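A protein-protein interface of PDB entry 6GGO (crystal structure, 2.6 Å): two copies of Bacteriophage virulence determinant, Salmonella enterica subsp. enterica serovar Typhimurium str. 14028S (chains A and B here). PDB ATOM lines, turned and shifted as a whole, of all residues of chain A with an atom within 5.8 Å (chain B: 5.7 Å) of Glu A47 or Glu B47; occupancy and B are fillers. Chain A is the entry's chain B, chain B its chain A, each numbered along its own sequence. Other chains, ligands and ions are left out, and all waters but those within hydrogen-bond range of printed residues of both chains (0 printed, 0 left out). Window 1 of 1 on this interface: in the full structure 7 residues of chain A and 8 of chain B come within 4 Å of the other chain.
The guanidinium group (NH2) of Arg A106 lies within salt-bridge range of the side-chain carboxylate (OE1) of Glu B47 (3.0 Å).
The side-chain sulfur (SG) of Cys B44 is disulfide-bonded to the side-chain sulfur (SG) of Cys A44 (2.0 Å).
The backbone carbonyl oxygen (O) of Met A43 sits close to the side-chain sulfur (SG) of Cys B44.
The guanidinium group of Arg B106 is in salt-bridge range of the side-chain carboxylate of Glu A47.
NH2 of Arg A71 lies within salt-bridge range of OE1 of Glu A47 (2.9 Å).
The guanidinium group (NE) of Arg B106 sits at hydrogen-bond distance from the backbone carbonyl oxygen (O) of Tyr B48.
The backbone carbonyl oxygen (O) of Glu B47 sits at hydrogen-bond distance from the guanidinium group (NH1) of Arg B106 (2.9 Å).
The side-chain carboxylate (OE2) of Glu B47 lies within salt-bridge range of the guanidinium group (NH2) of Arg B71, 3.1 Å away.
NE of Arg A106 lies within hydrogen-bond range of O of Tyr A48 (3.2 Å).
The guanidinium group of Arg A106 is in salt-bridge range of the side-chain carboxylate of Glu A47 (3.9 Å).
Cys A44 touches Met B43 (SG to C, 3.8 Å).
Glu B47 touches Glu A47 (CG to CG, 3.6 Å).
CE1 of Tyr B48 touches OE1 of Glu A47 (3.0 Å).
CE1 of Tyr A48 touches OE2 of Glu B47, 3.2 Å away.
Val B103 touches Ser A51.
CG2 of Val A103 touches O of Ser B51, at 3.2 Å.
CG1 of Val A103 touches CG1 of Val B103 (3.0 Å).
Glu A47 touches just these residues of chain B: Glu B47, Tyr B48 and Arg B106.
Of the printed residues of chain A, Met B43 touches Cys A44 (3.8 Å).
Of the printed residues of chain A, Arg B106 touches Glu A47 (2.9 Å).
Of the printed residues of chain B, Ser A51 touches Val B103 (2.9 Å).
Of the printed residues of chain A, Ser B51 touches Val A103 (3.2 Å).
The nearest residue of chain A that does not touch Glu B47 is Val A103 (4.5 Å).
Of the 13 printed residues of chain B, 7 touch a printed residue of chain A.
Of the 13 printed residues of chain A, 7 touch a printed residue of chain B.
Among the printed residues, Asp or Glu carboxylates within 4 Å of a Lys or Arg side-chain nitrogen of the other chain: Glu A47 with Arg B106 (2.9 Å) and Arg A106 with Glu B47 (3.0 Å).
Cys A44 touches its own counterpart, Cys B44.
Glu A47 touches its own counterpart, Glu B47.
Glu A47 touches Tyr B48, and with the chains exchanged Tyr A48 touches Glu B47.
Glu A47 touches Arg B106, and with the chains exchanged Arg A106 touches Glu B47.
13 positions are printed for both chains.
Of the 11 pairs that touch across the chains among the printed residues, 11 have their exchanged pair printed and touching as well.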
ATOM      1  N   MET A  43      23.459 -10.002  19.619  1.00  0.00           N
ATOM      2  CA  MET A  43      22.327 -10.800  20.074  1.00  0.00           C
ATOM      3  C   MET A  43      21.348 -10.002  20.925  1.00  0.00           C
ATOM      4  O   MET A  43      20.184 -10.398  21.040  1.00  0.00           O
ATOM      5  CB  MET A  43      22.827 -11.997  20.887  1.00  0.00           C
ATOM      6  CG  MET A  43      23.727 -12.961  20.131  1.00  0.00           C
ATOM      7  SD  MET A  43      22.816 -14.273  19.295  1.00  0.00           S
ATOM      8  CE  MET A  43      24.168 -15.296  18.715  1.00  0.00           C
ATOM      9  N   CYS A  44      21.788  -8.893  21.517  1.00  0.00           N
ATOM     10  CA  CYS A  44      20.978  -8.137  22.466  1.00  0.00           C
ATOM     11  C   CYS A  44      20.566  -6.770  21.937  1.00  0.00           C
ATOM     12  O   CYS A  44      20.068  -5.943  22.710  1.00  0.00           O
ATOM     13  CB  CYS A  44      21.734  -7.977  23.787  1.00  0.00           C
ATOM     14  SG  CYS A  44      22.693  -9.426  24.249  1.00  0.00           S
ATOM     15  N   LEU A  45      20.767  -6.505  20.645  1.00  0.00           N
ATOM     16  CA  LEU A  45      20.406  -5.199  20.107  1.00  0.00           C
ATOM     17  C   LEU A  45      18.909  -4.955  20.224  1.00  0.00           C
ATOM     18  O   LEU A  45      18.477  -3.830  20.496  1.00  0.00           O
ATOM     19  CB  LEU A  45      20.862  -5.089  18.655  1.00  0.00           C
ATOM     20  CG  LEU A  45      22.372  -5.205  18.429  1.00  0.00           C
ATOM     21  CD1 LEU A  45      22.695  -5.101  16.948  1.00  0.00           C
ATOM     22  CD2 LEU A  45      23.149  -4.155  19.224  1.00  0.00           C
ATOM     23  N   ALA A  46      18.100  -6.001  20.040  1.00  0.00           N
ATOM     24  CA  ALA A  46      16.656  -5.843  20.176  1.00  0.00           C
ATOM     25  C   ALA A  46      16.277  -5.385  21.579  1.00  0.00           C
ATOM     26  O   ALA A  46      15.382  -4.548  21.744  1.00  0.00           O
ATOM     27  CB  ALA A  46      15.951  -7.156  19.839  1.00  0.00           C
ATOM     28  N   GLU A  47      16.962  -5.907  22.603  1.00  0.00           N
ATOM     29  CA  GLU A  47      16.658  -5.521  23.979  1.00  0.00           C
ATOM     30  C   GLU A  47      17.104  -4.093  24.263  1.00  0.00           C
ATOM     31  O   GLU A  47      16.393  -3.337  24.937  1.00  0.00           O
ATOM     32  CB  GLU A  47      17.327  -6.491  24.955  1.00  0.00           C
ATOM     33  CG  GLU A  47      16.938  -6.304  26.423  1.00  0.00           C
ATOM     34  CD  GLU A  47      15.465  -6.567  26.694  1.00  0.00           C
ATOM     35  OE1 GLU A  47      14.983  -7.675  26.372  1.00  0.00           O
ATOM     36  OE2 GLU A  47      14.790  -5.671  27.245  1.00  0.00           O
ATOM     37  N   TYR A  48      18.279  -3.705  23.760  1.00  0.00           N
ATOM     38  CA  TYR A  48      18.739  -2.331  23.922  1.00  0.00           C
ATOM     39  C   TYR A  48      17.773  -1.347  23.280  1.00  0.00           C
ATOM     40  O   TYR A  48      17.627  -0.215  23.756  1.00  0.00           O
ATOM     41  CB  TYR A  48      20.135  -2.167  23.323  1.00  0.00           C
ATOM     42  CG  TYR A  48      21.201  -3.027  23.965  1.00  0.00           C
ATOM     43  CD1 TYR A  48      21.160  -3.335  25.322  1.00  0.00           C
ATOM     44  CD2 TYR A  48      22.254  -3.529  23.214  1.00  0.00           C
ATOM     45  CE1 TYR A  48      22.136  -4.118  25.907  1.00  0.00           C
ATOM     46  CE2 TYR A  48      23.234  -4.311  23.791  1.00  0.00           C
ATOM     47  CZ  TYR A  48      23.170  -4.604  25.138  1.00  0.00           C
ATOM     48  OH  TYR A  48      24.142  -5.384  25.716  1.00  0.00           O
ATOM     49  N   LEU A  49      17.130  -1.747  22.183  1.00  0.00           N
ATOM     50  CA  LEU A  49      16.239  -0.863  21.448  1.00  0.00           C
ATOM     51  C   LEU A  49      14.825  -0.858  22.014  1.00  0.00           C
ATOM     52  O   LEU A  49      14.199   0.204  22.099  1.00  0.00           O
ATOM     53  CB  LEU A  49      16.194  -1.272  19.972  1.00  0.00           C
ATOM     54  CG  LEU A  49      15.280  -0.429  19.082  1.00  0.00           C
ATOM     55  CD1 LEU A  49      15.821   0.983  18.972  1.00  0.00           C
ATOM     56  CD2 LEU A  49      15.126  -1.064  17.709  1.00  0.00           C
ATOM     57  N   ILE A  50      14.304  -2.019  22.399  1.00  0.00           N
ATOM     58  CA  ILE A  50      12.902  -2.168  22.766  1.00  0.00           C
ATOM     59  C   ILE A  50      12.803  -2.541  24.236  1.00  0.00           C
ATOM     60  O   ILE A  50      13.492  -3.457  24.700  1.00  0.00           O
ATOM     61  CB  ILE A  50      12.201  -3.221  21.890  1.00  0.00           C
ATOM     62  CG1 ILE A  50      12.184  -2.763  20.435  1.00  0.00           C
ATOM     63  CG2 ILE A  50      10.773  -3.466  22.375  1.00  0.00           C
ATOM     64  CD1 ILE A  50      11.823  -3.848  19.463  1.00  0.00           C
ATOM     65  N   SER A  51      11.948  -1.823  24.963  1.00  0.00           N
ATOM     66  CA  SER A  51      11.623  -2.185  26.336  1.00  0.00           C
ATOM     67  C   SER A  51      10.581  -3.298  26.371  1.00  0.00           C
ATOM     68  O   SER A  51      10.753  -4.301  27.072  1.00  0.00           O
ATOM     69  CB  SER A  51      11.121  -0.953  27.091  1.00  0.00           C
ATOM     70  OG  SER A  51       9.987  -0.397  26.450  1.00  0.00           O
ATOM     71  N   ARG A  71       9.381  -9.272  17.144  1.00  0.00           N
ATOM     72  CA  ARG A  71      10.613  -9.065  17.899  1.00  0.00           C
ATOM     73  C   ARG A  71      11.706 -10.033  17.463  1.00  0.00           C
ATOM     74  O   ARG A  71      12.886  -9.666  17.414  1.00  0.00           O
ATOM     75  CB  ARG A  71      10.328  -9.216  19.393  1.00  0.00           C
ATOM     76  CG  ARG A  71      11.404  -8.651  20.303  1.00  0.00           C
ATOM     77  CD  ARG A  71      11.109  -8.978  21.759  1.00  0.00           C
ATOM     78  NE  ARG A  71      11.744  -8.038  22.679  1.00  0.00           N
ATOM     79  CZ  ARG A  71      13.016  -8.099  23.059  1.00  0.00           C
ATOM     80  NH1 ARG A  71      13.812  -9.055  22.598  1.00  0.00           N
ATOM     81  NH2 ARG A  71      13.497  -7.196  23.903  1.00  0.00           N
ATOM     82  N   TYR A  96      23.163   4.424  21.406  1.00  0.00           N
ATOM     83  CA  TYR A  96      23.331   3.823  22.725  1.00  0.00           C
ATOM     84  C   TYR A  96      23.876   4.842  23.718  1.00  0.00           C
ATOM     85  O   TYR A  96      23.389   4.942  24.850  1.00  0.00           O
ATOM     86  CB  TYR A  96      24.250   2.605  22.630  1.00  0.00           C
ATOM     87  CG  TYR A  96      24.311   1.783  23.899  1.00  0.00           C
ATOM     88  CD1 TYR A  96      23.286   0.903  24.224  1.00  0.00           C
ATOM     89  CD2 TYR A  96      25.392   1.876  24.764  1.00  0.00           C
ATOM     90  CE1 TYR A  96      23.331   0.146  25.377  1.00  0.00           C
ATOM     91  CE2 TYR A  96      25.447   1.121  25.920  1.00  0.00           C
ATOM     92  CZ  TYR A  96      24.414   0.258  26.222  1.00  0.00           C
ATOM     93  OH  TYR A  96      24.460  -0.497  27.373  1.00  0.00           O
ATOM     94  N   VAL A 103      17.466   2.749  30.474  1.00  0.00           N
ATOM     95  CA  VAL A 103      16.424   1.772  30.200  1.00  0.00           C
ATOM     96  C   VAL A 103      15.072   2.446  29.990  1.00  0.00           C
ATOM     97  O   VAL A 103      14.244   1.952  29.216  1.00  0.00           O
ATOM     98  CB  VAL A 103      16.371   0.739  31.338  1.00  0.00           C
ATOM     99  CG1 VAL A 103      15.386  -0.342  31.011  1.00  0.00           C
ATOM    100  CG2 VAL A 103      17.749   0.135  31.582  1.00  0.00           C
ATOM    101  N   ARG A 106      13.970   3.688  26.128  1.00  0.00           N
ATOM    102  CA  ARG A 106      13.884   2.737  25.032  1.00  0.00           C
ATOM    103  C   ARG A 106      12.502   2.790  24.379  1.00  0.00           C
ATOM    104  O   ARG A 106      11.563   3.399  24.893  1.00  0.00           O
ATOM    105  CB  ARG A 106      14.197   1.326  25.531  1.00  0.00           C
ATOM    106  CG  ARG A 106      15.638   1.160  25.996  1.00  0.00           C
ATOM    107  CD  ARG A 106      15.936  -0.250  26.480  1.00  0.00           C
ATOM    108  NE  ARG A 106      17.324  -0.377  26.912  1.00  0.00           N
ATOM    109  CZ  ARG A 106      17.841  -1.463  27.478  1.00  0.00           C
ATOM    110  NH1 ARG A 106      17.085  -2.534  27.687  1.00  0.00           N
ATOM    111  NH2 ARG A 106      19.117  -1.480  27.836  1.00  0.00           N
ATOM    112  N   MET B  43      23.815 -14.370  26.314  1.00  0.00           N
ATOM    113  CA  MET B  43      24.619 -13.153  26.310  1.00  0.00           C
ATOM    114  C   MET B  43      23.864 -11.956  26.874  1.00  0.00           C
ATOM    115  O   MET B  43      24.497 -10.971  27.270  1.00  0.00           O
ATOM    116  CB  MET B  43      25.093 -12.843  24.890  1.00  0.00           C
ATOM    117  CG  MET B  43      25.983 -13.917  24.285  1.00  0.00           C
ATOM    118  SD  MET B  43      27.730 -13.656  24.645  1.00  0.00           S
ATOM    119  CE  MET B  43      28.479 -14.954  23.664  1.00  0.00           C
ATOM    120  N   CYS B  44      22.533 -12.017  26.919  1.00  0.00           N
ATOM    121  CA  CYS B  44      21.713 -10.880  27.314  1.00  0.00           C
ATOM    122  C   CYS B  44      21.015 -11.098  28.652  1.00  0.00           C
ATOM    123  O   CYS B  44      20.148 -10.303  29.025  1.00  0.00           O
ATOM    124  CB  CYS B  44      20.676 -10.592  26.227  1.00  0.00           C
ATOM    125  SG  CYS B  44      21.285 -10.866  24.542  1.00  0.00           S
ATOM    126  N   LEU B  45      21.370 -12.158  29.382  1.00  0.00           N
ATOM    127  CA  LEU B  45      20.718 -12.431  30.658  1.00  0.00           C
ATOM    128  C   LEU B  45      20.980 -11.317  31.664  1.00  0.00           C
ATOM    129  O   LEU B  45      20.098 -10.964  32.455  1.00  0.00           O
ATOM    130  CB  LEU B  45      21.193 -13.774  31.204  1.00  0.00           C
ATOM    131  CG  LEU B  45      20.874 -14.987  30.327  1.00  0.00           C
ATOM    132  CD1 LEU B  45      21.437 -16.247  30.952  1.00  0.00           C
ATOM    133  CD2 LEU B  45      19.375 -15.133  30.103  1.00  0.00           C
ATOM    134  N   ALA B  46      22.189 -10.748  31.647  1.00  0.00           N
ATOM    135  CA  ALA B  46      22.496  -9.637  32.540  1.00  0.00           C
ATOM    136  C   ALA B  46      21.571  -8.457  32.278  1.00  0.00           C
ATOM    137  O   ALA B  46      21.177  -7.746  33.210  1.00  0.00           O
ATOM    138  CB  ALA B  46      23.955  -9.217  32.375  1.00  0.00           C
ATOM    139  N   GLU B  47      21.227  -8.224  31.009  1.00  0.00           N
ATOM    140  CA  GLU B  47      20.329  -7.128  30.666  1.00  0.00           C
ATOM    141  C   GLU B  47      18.907  -7.422  31.128  1.00  0.00           C
ATOM    142  O   GLU B  47      18.204  -6.524  31.606  1.00  0.00           O
ATOM    143  CB  GLU B  47      20.364  -6.878  29.157  1.00  0.00           C
ATOM    144  CG  GLU B  47      19.638  -5.626  28.711  1.00  0.00           C
ATOM    145  CD  GLU B  47      20.269  -4.364  29.264  1.00  0.00           C
ATOM    146  OE1 GLU B  47      19.566  -3.592  29.950  1.00  0.00           O
ATOM    147  OE2 GLU B  47      21.475  -4.151  29.021  1.00  0.00           O
ATOM    148  N   TYR B  48      18.461  -8.673  30.981  1.00  0.00           N
ATOM    149  CA  TYR B  48      17.144  -9.048  31.485  1.00  0.00           C
ATOM    150  C   TYR B  48      17.053  -8.854  32.993  1.00  0.00           C
ATOM    151  O   TYR B  48      16.011  -8.436  33.512  1.00  0.00           O
ATOM    152  CB  TYR B  48      16.837 -10.508  31.147  1.00  0.00           C
ATOM    153  CG  TYR B  48      16.761 -10.852  29.677  1.00  0.00           C
ATOM    154  CD1 TYR B  48      16.278  -9.944  28.746  1.00  0.00           C
ATOM    155  CD2 TYR B  48      17.163 -12.102  29.223  1.00  0.00           C
ATOM    156  CE1 TYR B  48      16.203 -10.272  27.402  1.00  0.00           C
ATOM    157  CE2 TYR B  48      17.094 -12.438  27.887  1.00  0.00           C
ATOM    158  CZ  TYR B  48      16.613 -11.523  26.981  1.00  0.00           C
ATOM    159  OH  TYR B  48      16.549 -11.870  25.651  1.00  0.00           O
ATOM    160  N   LEU B  49      18.145  -9.133  33.711  1.00  0.00           N
ATOM    161  CA  LEU B  49      18.145  -9.117  35.172  1.00  0.00           C
ATOM    162  C   LEU B  49      18.384  -7.730  35.754  1.00  0.00           C
ATOM    163  O   LEU B  49      17.742  -7.361  36.743  1.00  0.00           O
ATOM    164  CB  LEU B  49      19.212 -10.076  35.705  1.00  0.00           C
ATOM    165  CG  LEU B  49      19.335 -10.181  37.234  1.00  0.00           C
ATOM    166  CD1 LEU B  49      18.091 -10.822  37.832  1.00  0.00           C
ATOM    167  CD2 LEU B  49      20.577 -10.952  37.641  1.00  0.00           C
ATOM    168  N   ILE B  50      19.307  -6.960  35.182  1.00  0.00           N
ATOM    169  CA  ILE B  50      19.746  -5.695  35.760  1.00  0.00           C
ATOM    170  C   ILE B  50      19.385  -4.563  34.809  1.00  0.00           C
ATOM    171  O   ILE B  50      19.682  -4.631  33.610  1.00  0.00           O
ATOM    172  CB  ILE B  50      21.257  -5.703  36.052  1.00  0.00           C
ATOM    173  CG1 ILE B  50      21.576  -6.761  37.105  1.00  0.00           C
ATOM    174  CG2 ILE B  50      21.721  -4.335  36.538  1.00  0.00           C
ATOM    175  CD1 ILE B  50      23.031  -7.074  37.220  1.00  0.00           C
ATOM    176  N   SER B  51      18.749  -3.524  35.349  1.00  0.00           N
ATOM    177  CA  SER B  51      18.494  -2.311  34.582  1.00  0.00           C
ATOM    178  C   SER B  51      19.725  -1.413  34.551  1.00  0.00           C
ATOM    179  O   SER B  51      20.127  -0.936  33.484  1.00  0.00           O
ATOM    180  CB  SER B  51      17.300  -1.563  35.173  1.00  0.00           C
ATOM    181  OG  SER B  51      17.531  -1.236  36.532  1.00  0.00           O
ATOM    182  N   ARG B  71      29.388  -6.120  36.487  1.00  0.00           N
ATOM    183  CA  ARG B  71      28.432  -6.525  35.460  1.00  0.00           C
ATOM    184  C   ARG B  71      29.078  -7.456  34.444  1.00  0.00           C
ATOM    185  O   ARG B  71      28.433  -8.383  33.944  1.00  0.00           O
ATOM    186  CB  ARG B  71      27.860  -5.294  34.762  1.00  0.00           C
ATOM    187  CG  ARG B  71      26.600  -5.575  33.954  1.00  0.00           C
ATOM    188  CD  ARG B  71      26.169  -4.363  33.145  1.00  0.00           C
ATOM    189  NE  ARG B  71      24.745  -4.386  32.811  1.00  0.00           N
ATOM    190  CZ  ARG B  71      24.215  -5.085  31.811  1.00  0.00           C
ATOM    191  NH1 ARG B  71      24.981  -5.840  31.036  1.00  0.00           N
ATOM    192  NH2 ARG B  71      22.909  -5.031  31.588  1.00  0.00           N
ATOM    193  N   TYR B  96      11.673 -14.775  34.215  1.00  0.00           N
ATOM    194  CA  TYR B  96      11.445 -13.898  33.068  1.00  0.00           C
ATOM    195  C   TYR B  96       9.958 -13.708  32.799  1.00  0.00           C
ATOM    196  O   TYR B  96       9.489 -12.577  32.621  1.00  0.00           O
ATOM    197  CB  TYR B  96      12.147 -14.469  31.835  1.00  0.00           C
ATOM    198  CG  TYR B  96      12.109 -13.568  30.621  1.00  0.00           C
ATOM    199  CD1 TYR B  96      12.965 -12.481  30.510  1.00  0.00           C
ATOM    200  CD2 TYR B  96      11.224 -13.814  29.578  1.00  0.00           C
ATOM    201  CE1 TYR B  96      12.933 -11.660  29.399  1.00  0.00           C
ATOM    202  CE2 TYR B  96      11.186 -13.001  28.467  1.00  0.00           C
ATOM    203  CZ  TYR B  96      12.042 -11.924  28.379  1.00  0.00           C
ATOM    204  OH  TYR B  96      12.007 -11.109  27.268  1.00  0.00           O
ATOM    205  N   VAL B 103      10.164  -4.367  32.106  1.00  0.00           N
ATOM    206  CA  VAL B 103      11.409  -3.635  32.269  1.00  0.00           C
ATOM    207  C   VAL B 103      11.459  -2.900  33.603  1.00  0.00           C
ATOM    208  O   VAL B 103      12.541  -2.712  34.169  1.00  0.00           O
ATOM    209  CB  VAL B 103      11.592  -2.684  31.076  1.00  0.00           C
ATOM    210  CG1 VAL B 103      12.913  -1.995  31.155  1.00  0.00           C
ATOM    211  CG2 VAL B 103      11.481  -3.459  29.767  1.00  0.00           C
ATOM    212  N   ARG B 106      12.992  -4.912  36.933  1.00  0.00           N
ATOM    213  CA  ARG B 106      14.346  -5.441  36.948  1.00  0.00           C
ATOM    214  C   ARG B 106      15.132  -4.887  38.134  1.00  0.00           C
ATOM    215  O   ARG B 106      14.716  -3.944  38.812  1.00  0.00           O
ATOM    216  CB  ARG B 106      15.050  -5.136  35.626  1.00  0.00           C
ATOM    217  CG  ARG B 106      14.440  -5.882  34.461  1.00  0.00           C
ATOM    218  CD  ARG B 106      15.145  -5.586  33.159  1.00  0.00           C
ATOM    219  NE  ARG B 106      14.544  -6.328  32.058  1.00  0.00           N
ATOM    220  CZ  ARG B 106      14.882  -6.185  30.783  1.00  0.00           C
ATOM    221  NH1 ARG B 106      15.826  -5.320  30.434  1.00  0.00           N
ATOM    222  NH2 ARG B 106      14.273  -6.909  29.858  1.00  0.00           N
